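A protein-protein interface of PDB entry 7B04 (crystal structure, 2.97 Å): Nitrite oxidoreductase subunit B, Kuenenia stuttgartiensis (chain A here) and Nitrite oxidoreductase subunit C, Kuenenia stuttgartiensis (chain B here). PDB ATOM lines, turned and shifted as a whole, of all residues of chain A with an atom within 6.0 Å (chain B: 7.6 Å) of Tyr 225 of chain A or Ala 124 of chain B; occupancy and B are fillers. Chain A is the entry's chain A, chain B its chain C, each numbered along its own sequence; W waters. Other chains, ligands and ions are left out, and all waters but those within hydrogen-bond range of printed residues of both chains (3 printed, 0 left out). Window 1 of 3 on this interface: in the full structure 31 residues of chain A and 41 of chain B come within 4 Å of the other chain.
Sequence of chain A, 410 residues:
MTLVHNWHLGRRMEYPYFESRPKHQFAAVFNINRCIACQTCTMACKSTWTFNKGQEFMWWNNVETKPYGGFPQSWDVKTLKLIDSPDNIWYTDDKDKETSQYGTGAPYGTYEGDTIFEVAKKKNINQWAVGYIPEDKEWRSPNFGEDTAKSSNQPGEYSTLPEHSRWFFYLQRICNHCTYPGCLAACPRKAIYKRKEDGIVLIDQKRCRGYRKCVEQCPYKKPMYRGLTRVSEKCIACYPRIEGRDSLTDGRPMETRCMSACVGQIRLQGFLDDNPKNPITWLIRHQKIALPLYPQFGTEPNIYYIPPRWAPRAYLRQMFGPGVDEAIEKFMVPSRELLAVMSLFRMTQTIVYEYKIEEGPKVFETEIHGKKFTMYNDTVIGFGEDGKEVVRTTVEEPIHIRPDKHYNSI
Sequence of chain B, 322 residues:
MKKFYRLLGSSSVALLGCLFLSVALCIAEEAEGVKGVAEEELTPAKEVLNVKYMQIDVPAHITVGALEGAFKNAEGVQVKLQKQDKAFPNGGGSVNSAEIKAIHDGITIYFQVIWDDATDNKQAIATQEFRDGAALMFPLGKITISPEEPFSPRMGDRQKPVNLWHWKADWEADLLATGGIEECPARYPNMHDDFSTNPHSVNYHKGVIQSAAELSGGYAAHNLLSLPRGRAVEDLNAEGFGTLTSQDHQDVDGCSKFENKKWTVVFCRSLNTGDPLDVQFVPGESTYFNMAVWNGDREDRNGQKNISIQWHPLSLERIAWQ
The guanidinium group of Arg 212 of chain A sits at hydrogen-bond distance from the backbone carbonyl oxygen of Ala 126 of chain B (3.4 Å). The guanidinium group of Arg 212 of chain A lies within hydrogen-bond range of the backbone carbonyl oxygen of Thr 127 of chain B (2.9 Å). The backbone carbonyl oxygen (O) of Glu 129 of chain B is in hydrogen-bond range of the guanidinium group (NH1) of Arg 212 of chain A (3.2 Å). The backbone carbonyl oxygen of Ala 124 of chain B is in hydrogen-bond range of the side-chain hydroxyl of Tyr 225 of chain A. NH2 of Arg 230 of chain A is in salt-bridge range of OD1 of Asp 174 of chain B, at 3.4 Å. The guanidinium group of Arg 230 of chain A is in hydrogen-bond range of the backbone carbonyl oxygen of Glu 182 of chain B (2.6 Å). The backbone carbonyl oxygen (O) of Thr 229 of chain A sits close to the backbone carbonyl oxygen (O) of Leu 225 of chain B, at 3.5 Å.
Among the printed residues, merely in contact across the chains: Arg 212 of chain A with Phe 130 of chain B (3.2 Å), Gly 227 of chain A with Ile 125 of chain B (3.3 Å), Arg 230 of chain A with Leu 225 of chain B (3.5 Å), Arg 230 of chain A with Ile 125 of chain B (3.7 Å), Tyr 225 of chain A with Ile 125 of chain B (3.8 Å), Phe 57 of chain A with Thr 127 of chain B (3.9 Å), Tyr 225 of chain A with Thr 127 of chain B (3.9 Å) and Tyr 225 of chain A with Ala 126 of chain B (3.9 Å).
Of the 18 printed residues of chain B, 9 touch a printed residue of chain A. Hydrophobic or aromatic side chains of chain B within 4 Å of the printed part of chain A: Ala 124, Ile 125 and Phe 130. Of the 17 printed residues of chain A, 6 touch a printed residue of chain B. Hydrophobic or aromatic side chains of chain A within 4 Å of the printed part of chain B: Phe 57 and Tyr 225. Among the printed residues, 15 pairs touch across the chains.
Of chain B, only Ala 124, Ile 125, Ala 126 and Thr 127 come within 4 Å of Tyr 225 of chain A. Ala 124 of chain B touches just one residue of chain A: Tyr 225. Of the printed residues of chain A, Glu 182 of chain B touches Arg 230 (2.6 Å). Of the printed residues of chain A, Asp 174 of chain B touches Arg 230 (3.4 Å). Of the printed residues of chain A, Ile 125 of chain B touches Tyr 225 (3.8 Å), Gly 227 (3.3 Å) and Arg 230 (3.7 Å). Arg 226 of chain A touches none of the printed residues of chain B. The nearest residue of chain B that does not touch Tyr 225 of chain A is Glu 129 of chain B (5.2 Å).
Water W2 lies within hydrogen-bond range of NH2 of Arg 230 of chain A (3.0 Å), OD1 of Asp 174 of chain B (3.1 Å) and OE1 of Glu 182 of chain B (3.1 Å). Water W3 bridges the backbone NH of Tyr 225 of chain A (3.1 Å) and the side-chain hydroxyl of Thr 127 of chain B (3.2 Å).
The backbone carbonyl oxygen of Gly 227 of chain A sits close to the guanidinium group of Arg 230 of chain A, at 3.4 Å. OE1 of Glu 182 of chain B lies within hydrogen-bond range of NE2 of Gln 123 of chain B (2.6 Å).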
ATOM      1  N   GLY A  54      33.004  11.922 -27.386  1.00  0.00           N
ATOM      2  CA  GLY A  54      31.654  12.283 -27.008  1.00  0.00           C
ATOM      3  C   GLY A  54      31.424  13.744 -26.695  1.00  0.00           C
ATOM      4  O   GLY A  54      30.263  14.162 -26.605  1.00  0.00           O
ATOM      5  N   PHE A  57      31.455  18.418 -29.684  1.00  0.00           N
ATOM      6  CA  PHE A  57      30.660  19.619 -29.886  1.00  0.00           C
ATOM      7  C   PHE A  57      30.574  20.487 -28.639  1.00  0.00           C
ATOM      8  O   PHE A  57      30.008  21.583 -28.703  1.00  0.00           O
ATOM      9  CB  PHE A  57      29.239  19.242 -30.319  1.00  0.00           C
ATOM     10  CG  PHE A  57      28.381  18.735 -29.191  1.00  0.00           C
ATOM     11  CD1 PHE A  57      28.483  17.421 -28.763  1.00  0.00           C
ATOM     12  CD2 PHE A  57      27.477  19.572 -28.553  1.00  0.00           C
ATOM     13  CE1 PHE A  57      27.702  16.951 -27.724  1.00  0.00           C
ATOM     14  CE2 PHE A  57      26.693  19.109 -27.513  1.00  0.00           C
ATOM     15  CZ  PHE A  57      26.805  17.795 -27.099  1.00  0.00           C
ATOM     16  N   MET A  58      31.120  20.029 -27.516  1.00  0.00           N
ATOM     17  CA  MET A  58      30.920  20.690 -26.232  1.00  0.00           C
ATOM     18  C   MET A  58      31.960  21.790 -26.047  1.00  0.00           C
ATOM     19  O   MET A  58      33.167  21.527 -26.095  1.00  0.00           O
ATOM     20  CB  MET A  58      30.993  19.675 -25.092  1.00  0.00           C
ATOM     21  CG  MET A  58      29.712  18.871 -24.916  1.00  0.00           C
ATOM     22  SD  MET A  58      29.896  17.384 -23.915  1.00  0.00           S
ATOM     23  CE  MET A  58      30.507  18.071 -22.382  1.00  0.00           C
ATOM     24  N   GLY A 210      20.930  10.821 -17.889  1.00  0.00           N
ATOM     25  CA  GLY A 210      20.742  11.351 -19.231  1.00  0.00           C
ATOM     26  C   GLY A 210      19.321  11.774 -19.533  1.00  0.00           C
ATOM     27  O   GLY A 210      18.808  11.492 -20.623  1.00  0.00           O
ATOM     28  N   TYR A 211      18.670  12.443 -18.583  1.00  0.00           N
ATOM     29  CA  TYR A 211      17.299  12.907 -18.743  1.00  0.00           C
ATOM     30  C   TYR A 211      17.179  14.164 -19.589  1.00  0.00           C
ATOM     31  O   TYR A 211      16.057  14.620 -19.808  1.00  0.00           O
ATOM     32  CB  TYR A 211      16.638  13.131 -17.384  1.00  0.00           C
ATOM     33  CG  TYR A 211      16.278  11.843 -16.680  1.00  0.00           C
ATOM     34  CD1 TYR A 211      16.353  10.618 -17.334  1.00  0.00           C
ATOM     35  CD2 TYR A 211      15.878  11.851 -15.356  1.00  0.00           C
ATOM     36  CE1 TYR A 211      16.033   9.439 -16.682  1.00  0.00           C
ATOM     37  CE2 TYR A 211      15.558  10.681 -14.702  1.00  0.00           C
ATOM     38  CZ  TYR A 211      15.637   9.479 -15.363  1.00  0.00           C
ATOM     39  OH  TYR A 211      15.314   8.317 -14.700  1.00  0.00           O
ATOM     40  N   ARG A 212      18.269  14.854 -19.897  1.00  0.00           N
ATOM     41  CA  ARG A 212      18.227  15.964 -20.844  1.00  0.00           C
ATOM     42  C   ARG A 212      17.296  17.095 -20.402  1.00  0.00           C
ATOM     43  O   ARG A 212      17.096  18.053 -21.159  1.00  0.00           O
ATOM     44  CB  ARG A 212      17.780  15.460 -22.233  1.00  0.00           C
ATOM     45  CG  ARG A 212      18.824  15.399 -23.341  1.00  0.00           C
ATOM     46  CD  ARG A 212      19.855  14.293 -23.153  1.00  0.00           C
ATOM     47  NE  ARG A 212      19.333  12.922 -23.194  1.00  0.00           N
ATOM     48  CZ  ARG A 212      19.242  12.171 -24.291  1.00  0.00           C
ATOM     49  NH1 ARG A 212      19.605  12.654 -25.471  1.00  0.00           N
ATOM     50  NH2 ARG A 212      18.770  10.933 -24.208  1.00  0.00           N
ATOM     51  N   VAL A 215      19.399  20.100 -19.931  1.00  0.00           N
ATOM     52  CA  VAL A 215      19.642  20.625 -21.271  1.00  0.00           C
ATOM     53  C   VAL A 215      18.409  21.344 -21.793  1.00  0.00           C
ATOM     54  O   VAL A 215      18.519  22.351 -22.504  1.00  0.00           O
ATOM     55  CB  VAL A 215      20.071  19.481 -22.213  1.00  0.00           C
ATOM     56  CG1 VAL A 215      20.365  20.010 -23.606  1.00  0.00           C
ATOM     57  CG2 VAL A 215      21.278  18.751 -21.644  1.00  0.00           C
ATOM     58  N   PRO A 223      24.366  22.991 -19.880  1.00  0.00           N
ATOM     59  CA  PRO A 223      24.388  21.525 -19.761  1.00  0.00           C
ATOM     60  C   PRO A 223      24.305  20.874 -21.132  1.00  0.00           C
ATOM     61  O   PRO A 223      23.435  21.205 -21.941  1.00  0.00           O
ATOM     62  CB  PRO A 223      23.149  21.209 -18.911  1.00  0.00           C
ATOM     63  CG  PRO A 223      22.785  22.484 -18.263  1.00  0.00           C
ATOM     64  CD  PRO A 223      23.168  23.549 -19.231  1.00  0.00           C
ATOM     65  N   MET A 224      25.212  19.937 -21.385  1.00  0.00           N
ATOM     66  CA  MET A 224      25.334  19.309 -22.689  1.00  0.00           C
ATOM     67  C   MET A 224      25.401  17.800 -22.524  1.00  0.00           C
ATOM     68  O   MET A 224      26.075  17.293 -21.624  1.00  0.00           O
ATOM     69  CB  MET A 224      26.571  19.821 -23.430  1.00  0.00           C
ATOM     70  CG  MET A 224      26.595  21.330 -23.597  1.00  0.00           C
ATOM     71  SD  MET A 224      28.179  21.976 -24.157  1.00  0.00           S
ATOM     72  CE  MET A 224      27.997  23.710 -23.749  1.00  0.00           C
ATOM     73  N   TYR A 225      24.704  17.088 -23.404  1.00  0.00           N
ATOM     74  CA  TYR A 225      24.600  15.636 -23.340  1.00  0.00           C
ATOM     75  C   TYR A 225      25.788  15.003 -24.047  1.00  0.00           C
ATOM     76  O   TYR A 225      26.057  15.298 -25.219  1.00  0.00           O
ATOM     77  CB  TYR A 225      23.289  15.177 -23.968  1.00  0.00           C
ATOM     78  CG  TYR A 225      23.066  13.681 -23.987  1.00  0.00           C
ATOM     79  CD1 TYR A 225      22.900  12.966 -22.808  1.00  0.00           C
ATOM     80  CD2 TYR A 225      22.991  12.989 -25.187  1.00  0.00           C
ATOM     81  CE1 TYR A 225      22.674  11.601 -22.825  1.00  0.00           C
ATOM     82  CE2 TYR A 225      22.771  11.625 -25.214  1.00  0.00           C
ATOM     83  CZ  TYR A 225      22.613  10.935 -24.031  1.00  0.00           C
ATOM     84  OH  TYR A 225      22.393   9.576 -24.060  1.00  0.00           O
ATOM     85  N   ARG A 226      26.493  14.137 -23.329  1.00  0.00           N
ATOM     86  CA  ARG A 226      27.658  13.444 -23.862  1.00  0.00           C
ATOM     87  C   ARG A 226      27.229  12.125 -24.484  1.00  0.00           C
ATOM     88  O   ARG A 226      26.805  11.206 -23.772  1.00  0.00           O
ATOM     89  CB  ARG A 226      28.702  13.205 -22.777  1.00  0.00           C
ATOM     90  CG  ARG A 226      30.056  12.825 -23.335  1.00  0.00           C
ATOM     91  CD  ARG A 226      31.136  12.794 -22.276  1.00  0.00           C
ATOM     92  NE  ARG A 226      32.342  12.170 -22.804  1.00  0.00           N
ATOM     93  CZ  ARG A 226      33.361  11.756 -22.061  1.00  0.00           C
ATOM     94  NH1 ARG A 226      33.334  11.881 -20.738  1.00  0.00           N
ATOM     95  NH2 ARG A 226      34.416  11.206 -22.646  1.00  0.00           N
ATOM     96  N   GLY A 227      27.245  12.078 -25.814  1.00  0.00           N
ATOM     97  CA  GLY A 227      26.875  10.857 -26.517  1.00  0.00           C
ATOM     98  C   GLY A 227      27.559   9.601 -26.007  1.00  0.00           C
ATOM     99  O   GLY A 227      26.928   8.550 -25.888  1.00  0.00           O
ATOM    100  N   THR A 229      28.947   8.817 -22.926  1.00  0.00           N
ATOM    101  CA  THR A 229      28.621   8.378 -21.573  1.00  0.00           C
ATOM    102  C   THR A 229      27.123   8.271 -21.324  1.00  0.00           C
ATOM    103  O   THR A 229      26.722   7.815 -20.247  1.00  0.00           O
ATOM    104  CB  THR A 229      29.246   9.333 -20.548  1.00  0.00           C
ATOM    105  OG1 THR A 229      28.846  10.679 -20.834  1.00  0.00           O
ATOM    106  CG2 THR A 229      30.764   9.237 -20.597  1.00  0.00           C
ATOM    107  N   ARG A 230      26.299   8.665 -22.293  1.00  0.00           N
ATOM    108  CA  ARG A 230      24.843   8.652 -22.188  1.00  0.00           C
ATOM    109  C   ARG A 230      24.337   9.458 -20.996  1.00  0.00           C
ATOM    110  O   ARG A 230      23.254   9.180 -20.471  1.00  0.00           O
ATOM    111  CB  ARG A 230      24.303   7.219 -22.118  1.00  0.00           C
ATOM    112  CG  ARG A 230      24.114   6.544 -23.469  1.00  0.00           C
ATOM    113  CD  ARG A 230      25.441   6.108 -24.068  1.00  0.00           C
ATOM    114  NE  ARG A 230      25.263   5.210 -25.204  1.00  0.00           N
ATOM    115  CZ  ARG A 230      26.251   4.795 -25.990  1.00  0.00           C
ATOM    116  NH1 ARG A 230      27.493   5.201 -25.767  1.00  0.00           N
ATOM    117  NH2 ARG A 230      25.998   3.977 -27.001  1.00  0.00           N
ATOM    118  N   VAL A 231      25.101  10.465 -20.563  1.00  0.00           N
ATOM    119  CA  VAL A 231      24.710  11.365 -19.485  1.00  0.00           C
ATOM    120  C   VAL A 231      25.173  12.767 -19.859  1.00  0.00           C
ATOM    121  O   VAL A 231      26.010  12.956 -20.744  1.00  0.00           O
ATOM    122  CB  VAL A 231      25.273  10.966 -18.098  1.00  0.00           C
ATOM    123  CG1 VAL A 231      24.980   9.504 -17.774  1.00  0.00           C
ATOM    124  CG2 VAL A 231      26.760  11.259 -18.015  1.00  0.00           C
ATOM    125  N   SER A 232      24.621  13.757 -19.165  1.00  0.00           N
ATOM    126  CA  SER A 232      24.943  15.152 -19.434  1.00  0.00           C
ATOM    127  C   SER A 232      26.050  15.655 -18.518  1.00  0.00           C
ATOM    128  O   SER A 232      26.238  15.164 -17.401  1.00  0.00           O
ATOM    129  CB  SER A 232      23.705  16.033 -19.269  1.00  0.00           C
ATOM    130  OG  SER A 232      22.689  15.669 -20.186  1.00  0.00           O
ATOM    131  N   GLU A 233      26.789  16.646 -19.011  1.00  0.00           N
ATOM    132  CA  GLU A 233      27.886  17.271 -18.290  1.00  0.00           C
ATOM    133  C   GLU A 233      27.739  18.783 -18.391  1.00  0.00           C
ATOM    134  O   GLU A 233      26.985  19.300 -19.220  1.00  0.00           O
ATOM    135  CB  GLU A 233      29.250  16.835 -18.842  1.00  0.00           C
ATOM    136  CG  GLU A 233      29.557  15.356 -18.679  1.00  0.00           C
ATOM    137  CD  GLU A 233      30.820  14.945 -19.413  1.00  0.00           C
ATOM    138  OE1 GLU A 233      31.344  15.763 -20.198  1.00  0.00           O
ATOM    139  OE2 GLU A 233      31.289  13.806 -19.204  1.00  0.00           O
ATOM    140  N   ASN B 121      13.514   3.079 -31.965  1.00  0.00           N
ATOM    141  CA  ASN B 121      14.517   3.966 -31.375  1.00  0.00           C
ATOM    142  C   ASN B 121      15.476   3.078 -30.594  1.00  0.00           C
ATOM    143  O   ASN B 121      15.161   2.622 -29.491  1.00  0.00           O
ATOM    144  CB  ASN B 121      13.876   5.025 -30.487  1.00  0.00           C
ATOM    145  CG  ASN B 121      12.826   5.841 -31.212  1.00  0.00           C
ATOM    146  OD1 ASN B 121      11.654   5.819 -30.835  1.00  0.00           O
ATOM    147  ND2 ASN B 121      13.236   6.581 -32.240  1.00  0.00           N
ATOM    148  N   LYS B 122      16.641   2.807 -31.178  1.00  0.00           N
ATOM    149  CA  LYS B 122      17.578   1.837 -30.629  1.00  0.00           C
ATOM    150  C   LYS B 122      18.878   2.455 -30.143  1.00  0.00           C
ATOM    151  O   LYS B 122      19.858   1.723 -29.933  1.00  0.00           O
ATOM    152  CB  LYS B 122      17.883   0.776 -31.685  1.00  0.00           C
ATOM    153  CG  LYS B 122      16.690  -0.077 -32.046  1.00  0.00           C
ATOM    154  CD  LYS B 122      17.047  -1.101 -33.093  1.00  0.00           C
ATOM    155  CE  LYS B 122      15.835  -1.932 -33.451  1.00  0.00           C
ATOM    156  NZ  LYS B 122      16.158  -2.948 -34.485  1.00  0.00           N
ATOM    157  N   GLN B 123      18.922   3.772 -29.955  1.00  0.00           N
ATOM    158  CA  GLN B 123      20.139   4.408 -29.470  1.00  0.00           C
ATOM    159  C   GLN B 123      19.817   5.833 -29.017  1.00  0.00           C
ATOM    160  O   GLN B 123      18.851   6.460 -29.467  1.00  0.00           O
ATOM    161  CB  GLN B 123      21.244   4.382 -30.535  1.00  0.00           C
ATOM    162  CG  GLN B 123      21.482   5.646 -31.306  1.00  0.00           C
ATOM    163  CD  GLN B 123      22.676   5.506 -32.238  1.00  0.00           C
ATOM    164  OE1 GLN B 123      22.951   6.395 -33.045  1.00  0.00           O
ATOM    165  NE2 GLN B 123      23.397   4.407 -32.118  1.00  0.00           N
ATOM    166  N   ALA B 124      20.667   6.339 -28.126  1.00  0.00           N
ATOM    167  CA  ALA B 124      20.509   7.650 -27.502  1.00  0.00           C
ATOM    168  C   ALA B 124      21.846   8.397 -27.468  1.00  0.00           C
ATOM    169  O   ALA B 124      22.316   8.880 -26.440  1.00  0.00           O
ATOM    170  CB  ALA B 124      19.905   7.513 -26.104  1.00  0.00           C
ATOM    171  N   ILE B 125      22.530   8.441 -28.606  1.00  0.00           N
ATOM    172  CA  ILE B 125      23.830   9.102 -28.698  1.00  0.00           C
ATOM    173  C   ILE B 125      23.685  10.568 -29.092  1.00  0.00           C
ATOM    174  O   ILE B 125      24.406  11.429 -28.587  1.00  0.00           O
ATOM    175  CB  ILE B 125      24.726   8.346 -29.707  1.00  0.00           C
ATOM    176  CG1 ILE B 125      25.096   6.960 -29.170  1.00  0.00           C
ATOM    177  CG2 ILE B 125      25.986   9.156 -30.012  1.00  0.00           C
ATOM    178  CD1 ILE B 125      26.175   6.259 -29.967  1.00  0.00           C
ATOM    179  N   ALA B 126      22.733  10.886 -29.958  1.00  0.00           N
ATOM    180  CA  ALA B 126      22.511  12.274 -30.340  1.00  0.00           C
ATOM    181  C   ALA B 126      21.685  12.975 -29.266  1.00  0.00           C
ATOM    182  O   ALA B 126      20.858  12.358 -28.587  1.00  0.00           O
ATOM    183  CB  ALA B 126      21.820  12.361 -31.700  1.00  0.00           C
ATOM    184  N   THR B 127      21.902  14.286 -29.133  1.00  0.00           N
ATOM    185  CA  THR B 127      21.292  15.039 -28.039  1.00  0.00           C
ATOM    186  C   THR B 127      19.766  15.027 -28.090  1.00  0.00           C
ATOM    187  O   THR B 127      19.105  15.030 -27.043  1.00  0.00           O
ATOM    188  CB  THR B 127      21.814  16.484 -28.060  1.00  0.00           C
ATOM    189  OG1 THR B 127      23.216  16.490 -27.782  1.00  0.00           O
ATOM    190  CG2 THR B 127      21.082  17.333 -27.034  1.00  0.00           C
ATOM    191  N   GLN B 128      19.190  14.968 -29.284  1.00  0.00           N
ATOM    192  CA  GLN B 128      17.741  15.028 -29.474  1.00  0.00           C
ATOM    193  C   GLN B 128      17.082  13.647 -29.527  1.00  0.00           C
ATOM    194  O   GLN B 128      15.872  13.559 -29.765  1.00  0.00           O
ATOM    195  CB  GLN B 128      17.394  15.846 -30.726  1.00  0.00           C
ATOM    196  CG  GLN B 128      17.732  15.191 -32.048  1.00  0.00           C
ATOM    197  CD  GLN B 128      19.201  15.302 -32.371  1.00  0.00           C
ATOM    198  OE1 GLN B 128      19.872  16.240 -31.942  1.00  0.00           O
ATOM    199  NE2 GLN B 128      19.715  14.336 -33.118  1.00  0.00           N
ATOM    200  N   GLU B 129      17.857  12.569 -29.425  1.00  0.00           N
ATOM    201  CA  GLU B 129      17.333  11.220 -29.584  1.00  0.00           C
ATOM    202  C   GLU B 129      17.273  10.489 -28.248  1.00  0.00           C
ATOM    203  O   GLU B 129      18.183  10.600 -27.416  1.00  0.00           O
ATOM    204  CB  GLU B 129      18.197  10.436 -30.574  1.00  0.00           C
ATOM    205  CG  GLU B 129      18.146  11.044 -31.953  1.00  0.00           C
ATOM    206  CD  GLU B 129      18.825  10.178 -32.993  1.00  0.00           C
ATOM    207  OE1 GLU B 129      19.633   9.311 -32.610  1.00  0.00           O
ATOM    208  OE2 GLU B 129      18.560  10.373 -34.191  1.00  0.00           O
ATOM    209  N   PHE B 130      16.230   9.687 -28.081  1.00  0.00           N
ATOM    210  CA  PHE B 130      15.991   8.934 -26.863  1.00  0.00           C
ATOM    211  C   PHE B 130      15.694   7.487 -27.225  1.00  0.00           C
ATOM    212  O   PHE B 130      15.420   7.151 -28.382  1.00  0.00           O
ATOM    213  CB  PHE B 130      14.826   9.530 -26.054  1.00  0.00           C
ATOM    214  CG  PHE B 130      15.032  10.962 -25.668  1.00  0.00           C
ATOM    215  CD1 PHE B 130      15.557  11.299 -24.435  1.00  0.00           C
ATOM    216  CD2 PHE B 130      14.707  11.981 -26.546  1.00  0.00           C
ATOM    217  CE1 PHE B 130      15.742  12.636 -24.083  1.00  0.00           C
ATOM    218  CE2 PHE B 130      14.892  13.310 -26.194  1.00  0.00           C
ATOM    219  CZ  PHE B 130      15.403  13.635 -24.965  1.00  0.00           C
ATOM    220  N   ARG B 131      15.692   6.633 -26.211  1.00  0.00           N
ATOM    221  CA  ARG B 131      15.585   5.202 -26.438  1.00  0.00           C
ATOM    222  C   ARG B 131      14.167   4.741 -26.142  1.00  0.00           C
ATOM    223  O   ARG B 131      13.480   5.287 -25.271  1.00  0.00           O
ATOM    224  CB  ARG B 131      16.554   4.423 -25.549  1.00  0.00           C
ATOM    225  CG  ARG B 131      16.283   4.701 -24.069  1.00  0.00           C
ATOM    226  CD  ARG B 131      16.996   3.712 -23.166  1.00  0.00           C
ATOM    227  NE  ARG B 131      18.395   4.069 -22.998  1.00  0.00           N
ATOM    228  CZ  ARG B 131      18.827   4.879 -22.038  1.00  0.00           C
ATOM    229  NH1 ARG B 131      17.970   5.420 -21.173  1.00  0.00           N
ATOM    230  NH2 ARG B 131      20.117   5.163 -21.952  1.00  0.00           N
ATOM    231  N   ASP B 132      13.748   3.697 -26.852  1.00  0.00           N
ATOM    232  CA  ASP B 132      12.548   2.971 -26.454  1.00  0.00           C
ATOM    233  C   ASP B 132      12.877   2.051 -25.294  1.00  0.00           C
ATOM    234  O   ASP B 132      13.930   1.415 -25.272  1.00  0.00           O
ATOM    235  CB  ASP B 132      11.974   2.163 -27.601  1.00  0.00           C
ATOM    236  CG  ASP B 132      11.236   3.023 -28.593  1.00  0.00           C
ATOM    237  OD1 ASP B 132      11.724   3.146 -29.726  1.00  0.00           O
ATOM    238  OD2 ASP B 132      10.186   3.593 -28.233  1.00  0.00           O
ATOM    239  N   ALA B 169      16.427  -0.380 -25.117  1.00  0.00           N
ATOM    240  CA  ALA B 169      16.639  -0.821 -26.492  1.00  0.00           C
ATOM    241  C   ALA B 169      18.070  -0.565 -26.943  1.00  0.00           C
ATOM    242  O   ALA B 169      18.646  -1.371 -27.683  1.00  0.00           O
ATOM    243  CB  ALA B 169      15.651  -0.128 -27.429  1.00  0.00           C
ATOM    244  N   ASP B 170      18.660   0.557 -26.519  1.00  0.00           N
ATOM    245  CA  ASP B 170      20.036   0.848 -26.904  1.00  0.00           C
ATOM    246  C   ASP B 170      21.009  -0.165 -26.317  1.00  0.00           C
ATOM    247  O   ASP B 170      22.035  -0.470 -26.936  1.00  0.00           O
ATOM    248  CB  ASP B 170      20.416   2.269 -26.481  1.00  0.00           C
ATOM    249  CG  ASP B 170      20.240   2.507 -24.994  1.00  0.00           C
ATOM    250  OD1 ASP B 170      19.734   1.605 -24.296  1.00  0.00           O
ATOM    251  OD2 ASP B 170      20.608   3.604 -24.523  1.00  0.00           O
ATOM    252  N   ASP B 174      23.989  -2.161 -27.969  1.00  0.00           N
ATOM    253  CA  ASP B 174      25.335  -2.158 -27.408  1.00  0.00           C
ATOM    254  C   ASP B 174      25.902  -3.566 -27.302  1.00  0.00           C
ATOM    255  O   ASP B 174      27.115  -3.758 -27.445  1.00  0.00           O
ATOM    256  CB  ASP B 174      25.333  -1.479 -26.038  1.00  0.00           C
ATOM    257  CG  ASP B 174      25.065   0.011 -26.126  1.00  0.00           C
ATOM    258  OD1 ASP B 174      25.403   0.617 -27.165  1.00  0.00           O
ATOM    259  OD2 ASP B 174      24.519   0.577 -25.156  1.00  0.00           O
ATOM    260  N   GLU B 182      28.051   1.076 -28.208  1.00  0.00           N
ATOM    261  CA  GLU B 182      28.152   1.891 -29.409  1.00  0.00           C
ATOM    262  C   GLU B 182      28.750   3.246 -29.060  1.00  0.00           C
ATOM    263  O   GLU B 182      28.350   3.876 -28.076  1.00  0.00           O
ATOM    264  CB  GLU B 182      26.781   2.071 -30.058  1.00  0.00           C
ATOM    265  CG  GLU B 182      26.271   0.849 -30.803  1.00  0.00           C
ATOM    266  CD  GLU B 182      24.922   1.088 -31.447  1.00  0.00           C
ATOM    267  OE1 GLU B 182      24.296   2.124 -31.144  1.00  0.00           O
ATOM    268  OE2 GLU B 182      24.486   0.240 -32.255  1.00  0.00           O
ATOM    269  N   ARG B 187      26.963   7.005 -34.816  1.00  0.00           N
ATOM    270  CA  ARG B 187      25.934   8.010 -35.046  1.00  0.00           C
ATOM    271  C   ARG B 187      26.363   9.080 -36.038  1.00  0.00           C
ATOM    272  O   ARG B 187      25.532   9.556 -36.819  1.00  0.00           O
ATOM    273  CB  ARG B 187      25.540   8.672 -33.719  1.00  0.00           C
ATOM    274  CG  ARG B 187      24.529   9.804 -33.844  1.00  0.00           C
ATOM    275  CD  ARG B 187      23.188   9.297 -34.341  1.00  0.00           C
ATOM    276  NE  ARG B 187      22.199  10.362 -34.445  1.00  0.00           N
ATOM    277  CZ  ARG B 187      22.043  11.128 -35.518  1.00  0.00           C
ATOM    278  NH1 ARG B 187      22.816  10.944 -36.580  1.00  0.00           N
ATOM    279  NH2 ARG B 187      21.118  12.077 -35.531  1.00  0.00           N
ATOM    280  N   LEU B 225      25.315   3.471 -17.307  1.00  0.00           N
ATOM    281  CA  LEU B 225      24.901   3.972 -18.615  1.00  0.00           C
ATOM    282  C   LEU B 225      26.083   4.329 -19.509  1.00  0.00           C
ATOM    283  O   LEU B 225      25.901   4.490 -20.722  1.00  0.00           O
ATOM    284  CB  LEU B 225      24.004   5.195 -18.451  1.00  0.00           C
ATOM    285  CG  LEU B 225      22.765   5.030 -17.577  1.00  0.00           C
ATOM    286  CD1 LEU B 225      21.956   6.301 -17.599  1.00  0.00           C
ATOM    287  CD2 LEU B 225      21.926   3.864 -18.061  1.00  0.00           C
HETATM  288  O   HOH W   1      23.698   2.858 -24.114  1.00  0.00           O
HETATM  289  O   HOH W   2      23.506   2.821 -28.177  1.00  0.00           O
HETATM  290  O   HOH W   3      23.547  18.882 -25.627  1.00  0.00           O
